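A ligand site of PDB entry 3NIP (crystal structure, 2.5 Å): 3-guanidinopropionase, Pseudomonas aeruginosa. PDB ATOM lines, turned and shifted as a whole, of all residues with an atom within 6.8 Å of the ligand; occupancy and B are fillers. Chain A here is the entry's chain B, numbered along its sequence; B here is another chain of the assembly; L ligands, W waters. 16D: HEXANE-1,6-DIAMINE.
N1 of the ligand sits close to NH1 of Arg 51 of chain B, at 3.5 Å.
O of Phe 248 is in hydrogen-bond range of N2 of the ligand.
O of Gly 292 lies within hydrogen-bond range of N1 of the ligand, at 2.8 Å.
The guanidinium group (NH2) of Arg 51 of chain B sits at hydrogen-bond distance from the backbone carbonyl oxygen (O) of Thr 252 of chain B.
Ala 294 touches the ligand (O to C5, 2.9 Å).
CD2 of Leu 297 touches C4 of the ligand, at 3.4 Å.
CG2 of Val 298 touches N2 of the ligand, 3.3 Å away.
Pro 246 of chain B touches the ligand (CB to C6, 3.0 Å).
Pro 250 of chain B touches the ligand (O to C1, 3.5 Å).
Pro 255 of chain B touches the ligand (CG to C2, 3.8 Å).
Ile 257 of chain B touches the ligand.
Hydrophobic or aromatic side chains within 4 Å of the ligand: Ala 294, Leu 297, Val 298, Pro 246 of chain B, Pro 255 of chain B and Ile 257 of chain B.
Ten residues have an atom within 4 Å of the ligand: Phe 248, Gly 292, Ala 294, Leu 297, Val 298, Arg 51 of chain B, Pro 246 of chain B, Pro 250 of chain B, Pro 255 of chain B and Ile 257 of chain B.
Water W2 lies within hydrogen-bond range of the side-chain hydroxyl (OG) of Ser 262 (2.6 Å), the side-chain carboxylate (OD2) of Asp 245 of chain B (2.8 Å) and a nitrogen (N2) of the ligand (2.8 Å).
Water W1 lies within hydrogen-bond range of the backbone carbonyl oxygen (O) of Ala 247 of chain A (2.7 Å) and a nitrogen (N2) of the ligand (3.0 Å).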
ATOM      1  N   LEU A  64       4.560 -18.049 -10.250  1.00  0.00           N
ATOM      2  CA  LEU A  64       5.038 -19.401 -10.033  1.00  0.00           C
ATOM      3  C   LEU A  64       6.445 -19.492  -9.446  1.00  0.00           C
ATOM      4  O   LEU A  64       6.831 -20.558  -8.957  1.00  0.00           O
ATOM      5  CB  LEU A  64       4.836 -20.234 -11.304  1.00  0.00           C
ATOM      6  CG  LEU A  64       3.304 -20.265 -11.420  1.00  0.00           C
ATOM      7  CD1 LEU A  64       2.753 -20.921 -12.692  1.00  0.00           C
ATOM      8  CD2 LEU A  64       2.643 -20.743 -10.134  1.00  0.00           C
ATOM      9  N   LEU A  67       7.342 -20.839  -5.865  1.00  0.00           N
ATOM     10  CA  LEU A  67       7.703 -22.222  -5.579  1.00  0.00           C
ATOM     11  C   LEU A  67       9.202 -22.435  -5.446  1.00  0.00           C
ATOM     12  O   LEU A  67       9.625 -23.467  -4.930  1.00  0.00           O
ATOM     13  CB  LEU A  67       7.120 -23.177  -6.630  1.00  0.00           C
ATOM     14  CG  LEU A  67       5.582 -23.164  -6.667  1.00  0.00           C
ATOM     15  CD1 LEU A  67       5.034 -24.106  -7.716  1.00  0.00           C
ATOM     16  CD2 LEU A  67       5.003 -23.507  -5.277  1.00  0.00           C
ATOM     17  N   LEU A 244      11.916 -26.504 -25.529  1.00  0.00           N
ATOM     18  CA  LEU A 244      11.407 -27.651 -24.811  1.00  0.00           C
ATOM     19  C   LEU A 244      10.289 -28.289 -25.588  1.00  0.00           C
ATOM     20  O   LEU A 244       9.575 -27.600 -26.337  1.00  0.00           O
ATOM     21  CB  LEU A 244      10.862 -27.225 -23.461  1.00  0.00           C
ATOM     22  CG  LEU A 244      11.889 -26.785 -22.447  1.00  0.00           C
ATOM     23  CD1 LEU A 244      11.190 -26.080 -21.316  1.00  0.00           C
ATOM     24  CD2 LEU A 244      12.658 -27.997 -21.964  1.00  0.00           C
ATOM     25  N   ALA A 247       5.234 -30.886 -24.322  1.00  0.00           N
ATOM     26  CA  ALA A 247       4.811 -31.588 -23.106  1.00  0.00           C
ATOM     27  C   ALA A 247       5.295 -30.878 -21.852  1.00  0.00           C
ATOM     28  O   ALA A 247       4.640 -30.908 -20.817  1.00  0.00           O
ATOM     29  CB  ALA A 247       5.338 -33.022 -23.114  1.00  0.00           C
ATOM     30  N   PHE A 248       6.468 -30.265 -21.936  1.00  0.00           N
ATOM     31  CA  PHE A 248       7.062 -29.580 -20.805  1.00  0.00           C
ATOM     32  C   PHE A 248       6.784 -28.079 -20.873  1.00  0.00           C
ATOM     33  O   PHE A 248       6.756 -27.425 -19.842  1.00  0.00           O
ATOM     34  CB  PHE A 248       8.571 -29.852 -20.734  1.00  0.00           C
ATOM     35  CG  PHE A 248       8.931 -31.299 -20.908  1.00  0.00           C
ATOM     36  CD1 PHE A 248       8.915 -32.174 -19.816  1.00  0.00           C
ATOM     37  CD2 PHE A 248       9.289 -31.802 -22.160  1.00  0.00           C
ATOM     38  CE1 PHE A 248       9.237 -33.531 -19.977  1.00  0.00           C
ATOM     39  CE2 PHE A 248       9.603 -33.157 -22.342  1.00  0.00           C
ATOM     40  CZ  PHE A 248       9.586 -34.023 -21.254  1.00  0.00           C
ATOM     41  N   ALA A 249       6.559 -27.548 -22.078  1.00  0.00           N
ATOM     42  CA  ALA A 249       6.228 -26.135 -22.272  1.00  0.00           C
ATOM     43  C   ALA A 249       5.075 -25.937 -23.252  1.00  0.00           C
ATOM     44  O   ALA A 249       5.293 -25.552 -24.397  1.00  0.00           O
ATOM     45  CB  ALA A 249       7.453 -25.352 -22.756  1.00  0.00           C
ATOM     46  N   PRO A 250       3.837 -26.180 -22.802  1.00  0.00           N
ATOM     47  CA  PRO A 250       2.743 -25.937 -23.734  1.00  0.00           C
ATOM     48  C   PRO A 250       2.479 -24.443 -23.948  1.00  0.00           C
ATOM     49  O   PRO A 250       1.983 -24.037 -25.007  1.00  0.00           O
ATOM     50  CB  PRO A 250       1.542 -26.589 -23.047  1.00  0.00           C
ATOM     51  CG  PRO A 250       1.889 -26.615 -21.589  1.00  0.00           C
ATOM     52  CD  PRO A 250       3.375 -26.627 -21.468  1.00  0.00           C
ATOM     53  N   SER A 262      12.707 -30.834 -19.891  1.00  0.00           N
ATOM     54  CA  SER A 262      13.141 -29.969 -18.778  1.00  0.00           C
ATOM     55  C   SER A 262      14.427 -30.492 -18.143  1.00  0.00           C
ATOM     56  O   SER A 262      15.323 -29.717 -17.838  1.00  0.00           O
ATOM     57  CB  SER A 262      12.075 -29.909 -17.686  1.00  0.00           C
ATOM     58  OG  SER A 262      10.853 -29.470 -18.218  1.00  0.00           O
ATOM     59  N   VAL A 291      -1.021 -24.308 -19.488  1.00  0.00           N
ATOM     60  CA  VAL A 291      -1.910 -25.209 -18.787  1.00  0.00           C
ATOM     61  C   VAL A 291      -1.476 -25.252 -17.326  1.00  0.00           C
ATOM     62  O   VAL A 291      -0.380 -25.723 -17.008  1.00  0.00           O
ATOM     63  CB  VAL A 291      -1.865 -26.617 -19.392  1.00  0.00           C
ATOM     64  CG1 VAL A 291      -2.951 -27.462 -18.790  1.00  0.00           C
ATOM     65  CG2 VAL A 291      -2.001 -26.558 -20.928  1.00  0.00           C
ATOM     66  N   GLY A 292      -2.324 -24.728 -16.450  1.00  0.00           N
ATOM     67  CA  GLY A 292      -2.055 -24.702 -15.014  1.00  0.00           C
ATOM     68  C   GLY A 292      -0.732 -24.069 -14.606  1.00  0.00           C
ATOM     69  O   GLY A 292      -0.096 -24.500 -13.650  1.00  0.00           O
ATOM     70  N   GLY A 293      -0.317 -23.040 -15.334  1.00  0.00           N
ATOM     71  CA  GLY A 293       0.986 -22.409 -15.082  1.00  0.00           C
ATOM     72  C   GLY A 293       2.202 -23.297 -15.300  1.00  0.00           C
ATOM     73  O   GLY A 293       3.289 -23.000 -14.785  1.00  0.00           O
ATOM     74  N   ALA A 294       2.051 -24.376 -16.056  1.00  0.00           N
ATOM     75  CA  ALA A 294       3.150 -25.288 -16.315  1.00  0.00           C
ATOM     76  C   ALA A 294       4.382 -24.577 -16.865  1.00  0.00           C
ATOM     77  O   ALA A 294       5.491 -24.744 -16.343  1.00  0.00           O
ATOM     78  CB  ALA A 294       2.729 -26.449 -17.253  1.00  0.00           C
ATOM     79  N   THR A 295       4.163 -23.767 -17.901  1.00  0.00           N
ATOM     80  CA  THR A 295       5.247 -23.099 -18.588  1.00  0.00           C
ATOM     81  C   THR A 295       5.840 -21.973 -17.750  1.00  0.00           C
ATOM     82  O   THR A 295       7.046 -21.764 -17.765  1.00  0.00           O
ATOM     83  CB  THR A 295       4.821 -22.613 -19.978  1.00  0.00           C
ATOM     84  OG1 THR A 295       4.052 -23.649 -20.607  1.00  0.00           O
ATOM     85  CG2 THR A 295       6.038 -22.316 -20.836  1.00  0.00           C
ATOM     86  N   ALA A 296       4.989 -21.288 -16.981  1.00  0.00           N
ATOM     87  CA  ALA A 296       5.450 -20.264 -16.035  1.00  0.00           C
ATOM     88  C   ALA A 296       6.380 -20.854 -14.978  1.00  0.00           C
ATOM     89  O   ALA A 296       7.405 -20.260 -14.651  1.00  0.00           O
ATOM     90  CB  ALA A 296       4.259 -19.580 -15.380  1.00  0.00           C
ATOM     91  N   LEU A 297       6.057 -22.052 -14.480  1.00  0.00           N
ATOM     92  CA  LEU A 297       6.929 -22.775 -13.549  1.00  0.00           C
ATOM     93  C   LEU A 297       8.254 -23.121 -14.193  1.00  0.00           C
ATOM     94  O   LEU A 297       9.312 -22.822 -13.618  1.00  0.00           O
ATOM     95  CB  LEU A 297       6.248 -24.026 -12.979  1.00  0.00           C
ATOM     96  CG  LEU A 297       7.095 -24.790 -11.912  1.00  0.00           C
ATOM     97  CD1 LEU A 297       7.593 -23.894 -10.760  1.00  0.00           C
ATOM     98  CD2 LEU A 297       6.352 -25.992 -11.347  1.00  0.00           C
ATOM     99  N   VAL A 298       8.213 -23.734 -15.376  1.00  0.00           N
ATOM    100  CA  VAL A 298       9.425 -23.994 -16.136  1.00  0.00           C
ATOM    101  C   VAL A 298      10.219 -22.689 -16.235  1.00  0.00           C
ATOM    102  O   VAL A 298      11.391 -22.644 -15.862  1.00  0.00           O
ATOM    103  CB  VAL A 298       9.135 -24.513 -17.555  1.00  0.00           C
ATOM    104  CG1 VAL A 298      10.422 -24.597 -18.369  1.00  0.00           C
ATOM    105  CG2 VAL A 298       8.441 -25.889 -17.507  1.00  0.00           C
ATOM    106  N   ARG B  51       0.175 -25.972  -1.782  1.00  0.00           N
ATOM    107  CA  ARG B  51      -0.941 -26.300  -2.674  1.00  0.00           C
ATOM    108  C   ARG B  51      -1.613 -27.611  -2.248  1.00  0.00           C
ATOM    109  O   ARG B  51      -1.021 -28.686  -2.340  1.00  0.00           O
ATOM    110  CB  ARG B  51      -0.505 -26.374  -4.155  1.00  0.00           C
ATOM    111  CG  ARG B  51       0.214 -25.115  -4.687  1.00  0.00           C
ATOM    112  CD  ARG B  51       0.210 -25.030  -6.202  1.00  0.00           C
ATOM    113  NE  ARG B  51       0.684 -26.250  -6.853  1.00  0.00           N
ATOM    114  CZ  ARG B  51       0.762 -26.433  -8.166  1.00  0.00           C
ATOM    115  NH1 ARG B  51       0.397 -25.477  -9.020  1.00  0.00           N
ATOM    116  NH2 ARG B  51       1.195 -27.603  -8.641  1.00  0.00           N
ATOM    117  N   ASP B 245       7.989 -36.219 -13.884  1.00  0.00           N
ATOM    118  CA  ASP B 245       7.946 -34.890 -14.437  1.00  0.00           C
ATOM    119  C   ASP B 245       6.508 -34.367 -14.464  1.00  0.00           C
ATOM    120  O   ASP B 245       5.554 -35.136 -14.674  1.00  0.00           O
ATOM    121  CB  ASP B 245       8.598 -34.828 -15.831  1.00  0.00           C
ATOM    122  CG  ASP B 245       9.026 -33.395 -16.198  1.00  0.00           C
ATOM    123  OD1 ASP B 245      10.212 -33.076 -15.977  1.00  0.00           O
ATOM    124  OD2 ASP B 245       8.181 -32.593 -16.639  1.00  0.00           O
ATOM    125  N   PRO B 246       6.326 -33.072 -14.210  1.00  0.00           N
ATOM    126  CA  PRO B 246       5.014 -32.442 -14.332  1.00  0.00           C
ATOM    127  C   PRO B 246       4.305 -32.714 -15.654  1.00  0.00           C
ATOM    128  O   PRO B 246       3.088 -32.662 -15.716  1.00  0.00           O
ATOM    129  CB  PRO B 246       5.346 -30.968 -14.231  1.00  0.00           C
ATOM    130  CG  PRO B 246       6.501 -30.940 -13.259  1.00  0.00           C
ATOM    131  CD  PRO B 246       7.295 -32.186 -13.523  1.00  0.00           C
ATOM    132  N   ALA B 247       5.079 -32.988 -16.703  1.00  0.00           N
ATOM    133  CA  ALA B 247       4.538 -33.374 -18.005  1.00  0.00           C
ATOM    134  C   ALA B 247       3.692 -34.630 -17.915  1.00  0.00           C
ATOM    135  O   ALA B 247       2.716 -34.796 -18.648  1.00  0.00           O
ATOM    136  CB  ALA B 247       5.684 -33.591 -19.016  1.00  0.00           C
ATOM    137  N   ALA B 249       2.827 -35.897 -14.618  1.00  0.00           N
ATOM    138  CA  ALA B 249       1.974 -35.742 -13.431  1.00  0.00           C
ATOM    139  C   ALA B 249       1.691 -34.278 -13.050  1.00  0.00           C
ATOM    140  O   ALA B 249       2.200 -33.791 -12.041  1.00  0.00           O
ATOM    141  CB  ALA B 249       2.570 -36.516 -12.230  1.00  0.00           C
ATOM    142  N   PRO B 250       0.869 -33.565 -13.832  1.00  0.00           N
ATOM    143  CA  PRO B 250       0.662 -32.147 -13.490  1.00  0.00           C
ATOM    144  C   PRO B 250      -0.135 -31.949 -12.181  1.00  0.00           C
ATOM    145  O   PRO B 250       0.059 -30.964 -11.475  1.00  0.00           O
ATOM    146  CB  PRO B 250      -0.121 -31.596 -14.682  1.00  0.00           C
ATOM    147  CG  PRO B 250      -0.792 -32.763 -15.274  1.00  0.00           C
ATOM    148  CD  PRO B 250       0.079 -33.979 -15.017  1.00  0.00           C
ATOM    149  N   GLY B 251      -1.012 -32.892 -11.861  1.00  0.00           N
ATOM    150  CA  GLY B 251      -1.899 -32.740 -10.704  1.00  0.00           C
ATOM    151  C   GLY B 251      -1.241 -33.156  -9.407  1.00  0.00           C
ATOM    152  O   GLY B 251      -1.519 -34.233  -8.888  1.00  0.00           O
ATOM    153  N   THR B 252      -0.358 -32.285  -8.899  1.00  0.00           N
ATOM    154  CA  THR B 252       0.357 -32.522  -7.649  1.00  0.00           C
ATOM    155  C   THR B 252       0.755 -31.193  -7.002  1.00  0.00           C
ATOM    156  O   THR B 252       1.023 -30.213  -7.699  1.00  0.00           O
ATOM    157  CB  THR B 252       1.555 -33.485  -7.861  1.00  0.00           C
ATOM    158  OG1 THR B 252       1.899 -34.128  -6.625  1.00  0.00           O
ATOM    159  CG2 THR B 252       2.776 -32.775  -8.465  1.00  0.00           C
ATOM    160  N   PRO B 255       5.250 -29.623  -7.366  1.00  0.00           N
ATOM    161  CA  PRO B 255       5.979 -30.155  -8.528  1.00  0.00           C
ATOM    162  C   PRO B 255       7.422 -29.619  -8.622  1.00  0.00           C
ATOM    163  O   PRO B 255       7.695 -28.498  -8.216  1.00  0.00           O
ATOM    164  CB  PRO B 255       5.146 -29.660  -9.720  1.00  0.00           C
ATOM    165  CG  PRO B 255       4.530 -28.381  -9.219  1.00  0.00           C
ATOM    166  CD  PRO B 255       4.288 -28.582  -7.741  1.00  0.00           C
ATOM    167  N   GLU B 256       8.322 -30.458  -9.119  1.00  0.00           N
ATOM    168  CA  GLU B 256       9.678 -30.035  -9.442  1.00  0.00           C
ATOM    169  C   GLU B 256       9.935 -30.479 -10.877  1.00  0.00           C
ATOM    170  O   GLU B 256       9.853 -31.674 -11.196  1.00  0.00           O
ATOM    171  CB  GLU B 256      10.711 -30.695  -8.509  1.00  0.00           C
ATOM    172  CG  GLU B 256      10.379 -30.649  -7.004  1.00  0.00           C
ATOM    173  CD  GLU B 256      10.582 -29.271  -6.395  1.00  0.00           C
ATOM    174  OE1 GLU B 256      11.285 -28.445  -7.022  1.00  0.00           O
ATOM    175  OE2 GLU B 256      10.053 -29.007  -5.300  1.00  0.00           O
ATOM    176  N   ILE B 257      10.244 -29.531 -11.757  1.00  0.00           N
ATOM    177  CA  ILE B 257      10.519 -29.920 -13.140  1.00  0.00           C
ATOM    178  C   ILE B 257      11.744 -30.827 -13.199  1.00  0.00           C
ATOM    179  O   ILE B 257      12.474 -30.955 -12.207  1.00  0.00           O
ATOM    180  CB  ILE B 257      10.677 -28.697 -14.097  1.00  0.00           C
ATOM    181  CG1 ILE B 257      12.000 -27.970 -13.827  1.00  0.00           C
ATOM    182  CG2 ILE B 257       9.442 -27.770 -14.043  1.00  0.00           C
ATOM    183  CD1 ILE B 257      12.398 -27.028 -14.936  1.00  0.00           C
ATOM    184  N   PHE B 289      -5.389 -29.551  -9.348  1.00  0.00           N
ATOM    185  CA  PHE B 289      -4.291 -29.163 -10.261  1.00  0.00           C
ATOM    186  C   PHE B 289      -4.080 -30.122 -11.443  1.00  0.00           C
ATOM    187  O   PHE B 289      -3.182 -29.900 -12.261  1.00  0.00           O
ATOM    188  CB  PHE B 289      -2.985 -28.948  -9.479  1.00  0.00           C
ATOM    189  CG  PHE B 289      -3.077 -27.852  -8.474  1.00  0.00           C
ATOM    190  CD1 PHE B 289      -2.933 -26.520  -8.865  1.00  0.00           C
ATOM    191  CD2 PHE B 289      -3.376 -28.136  -7.134  1.00  0.00           C
ATOM    192  CE1 PHE B 289      -3.055 -25.481  -7.940  1.00  0.00           C
ATOM    193  CE2 PHE B 289      -3.501 -27.128  -6.206  1.00  0.00           C
ATOM    194  CZ  PHE B 289      -3.348 -25.789  -6.604  1.00  0.00           C
HETATM  195  N1  16D L   1       1.303 -26.399 -12.224  1.00  0.00           N
HETATM  196  C1  16D L   1       1.468 -27.871 -12.176  1.00  0.00           C
HETATM  197  C2  16D L   1       2.848 -28.377 -12.666  1.00  0.00           C
HETATM  198  C3  16D L   1       3.355 -27.908 -14.031  1.00  0.00           C
HETATM  199  C4  16D L   1       4.873 -27.581 -13.958  1.00  0.00           C
HETATM  200  C5  16D L   1       5.747 -27.407 -15.219  1.00  0.00           C
HETATM  201  C6  16D L   1       5.859 -28.667 -16.100  1.00  0.00           C
HETATM  202  N2  16D L   1       6.400 -28.506 -17.451  1.00  0.00           N
HETATM  203  O   HOH W   1       3.977 -30.048 -18.378  1.00  0.00           O
HETATM  204  O   HOH W   2       8.743 -29.889 -16.769  1.00  0.00           O
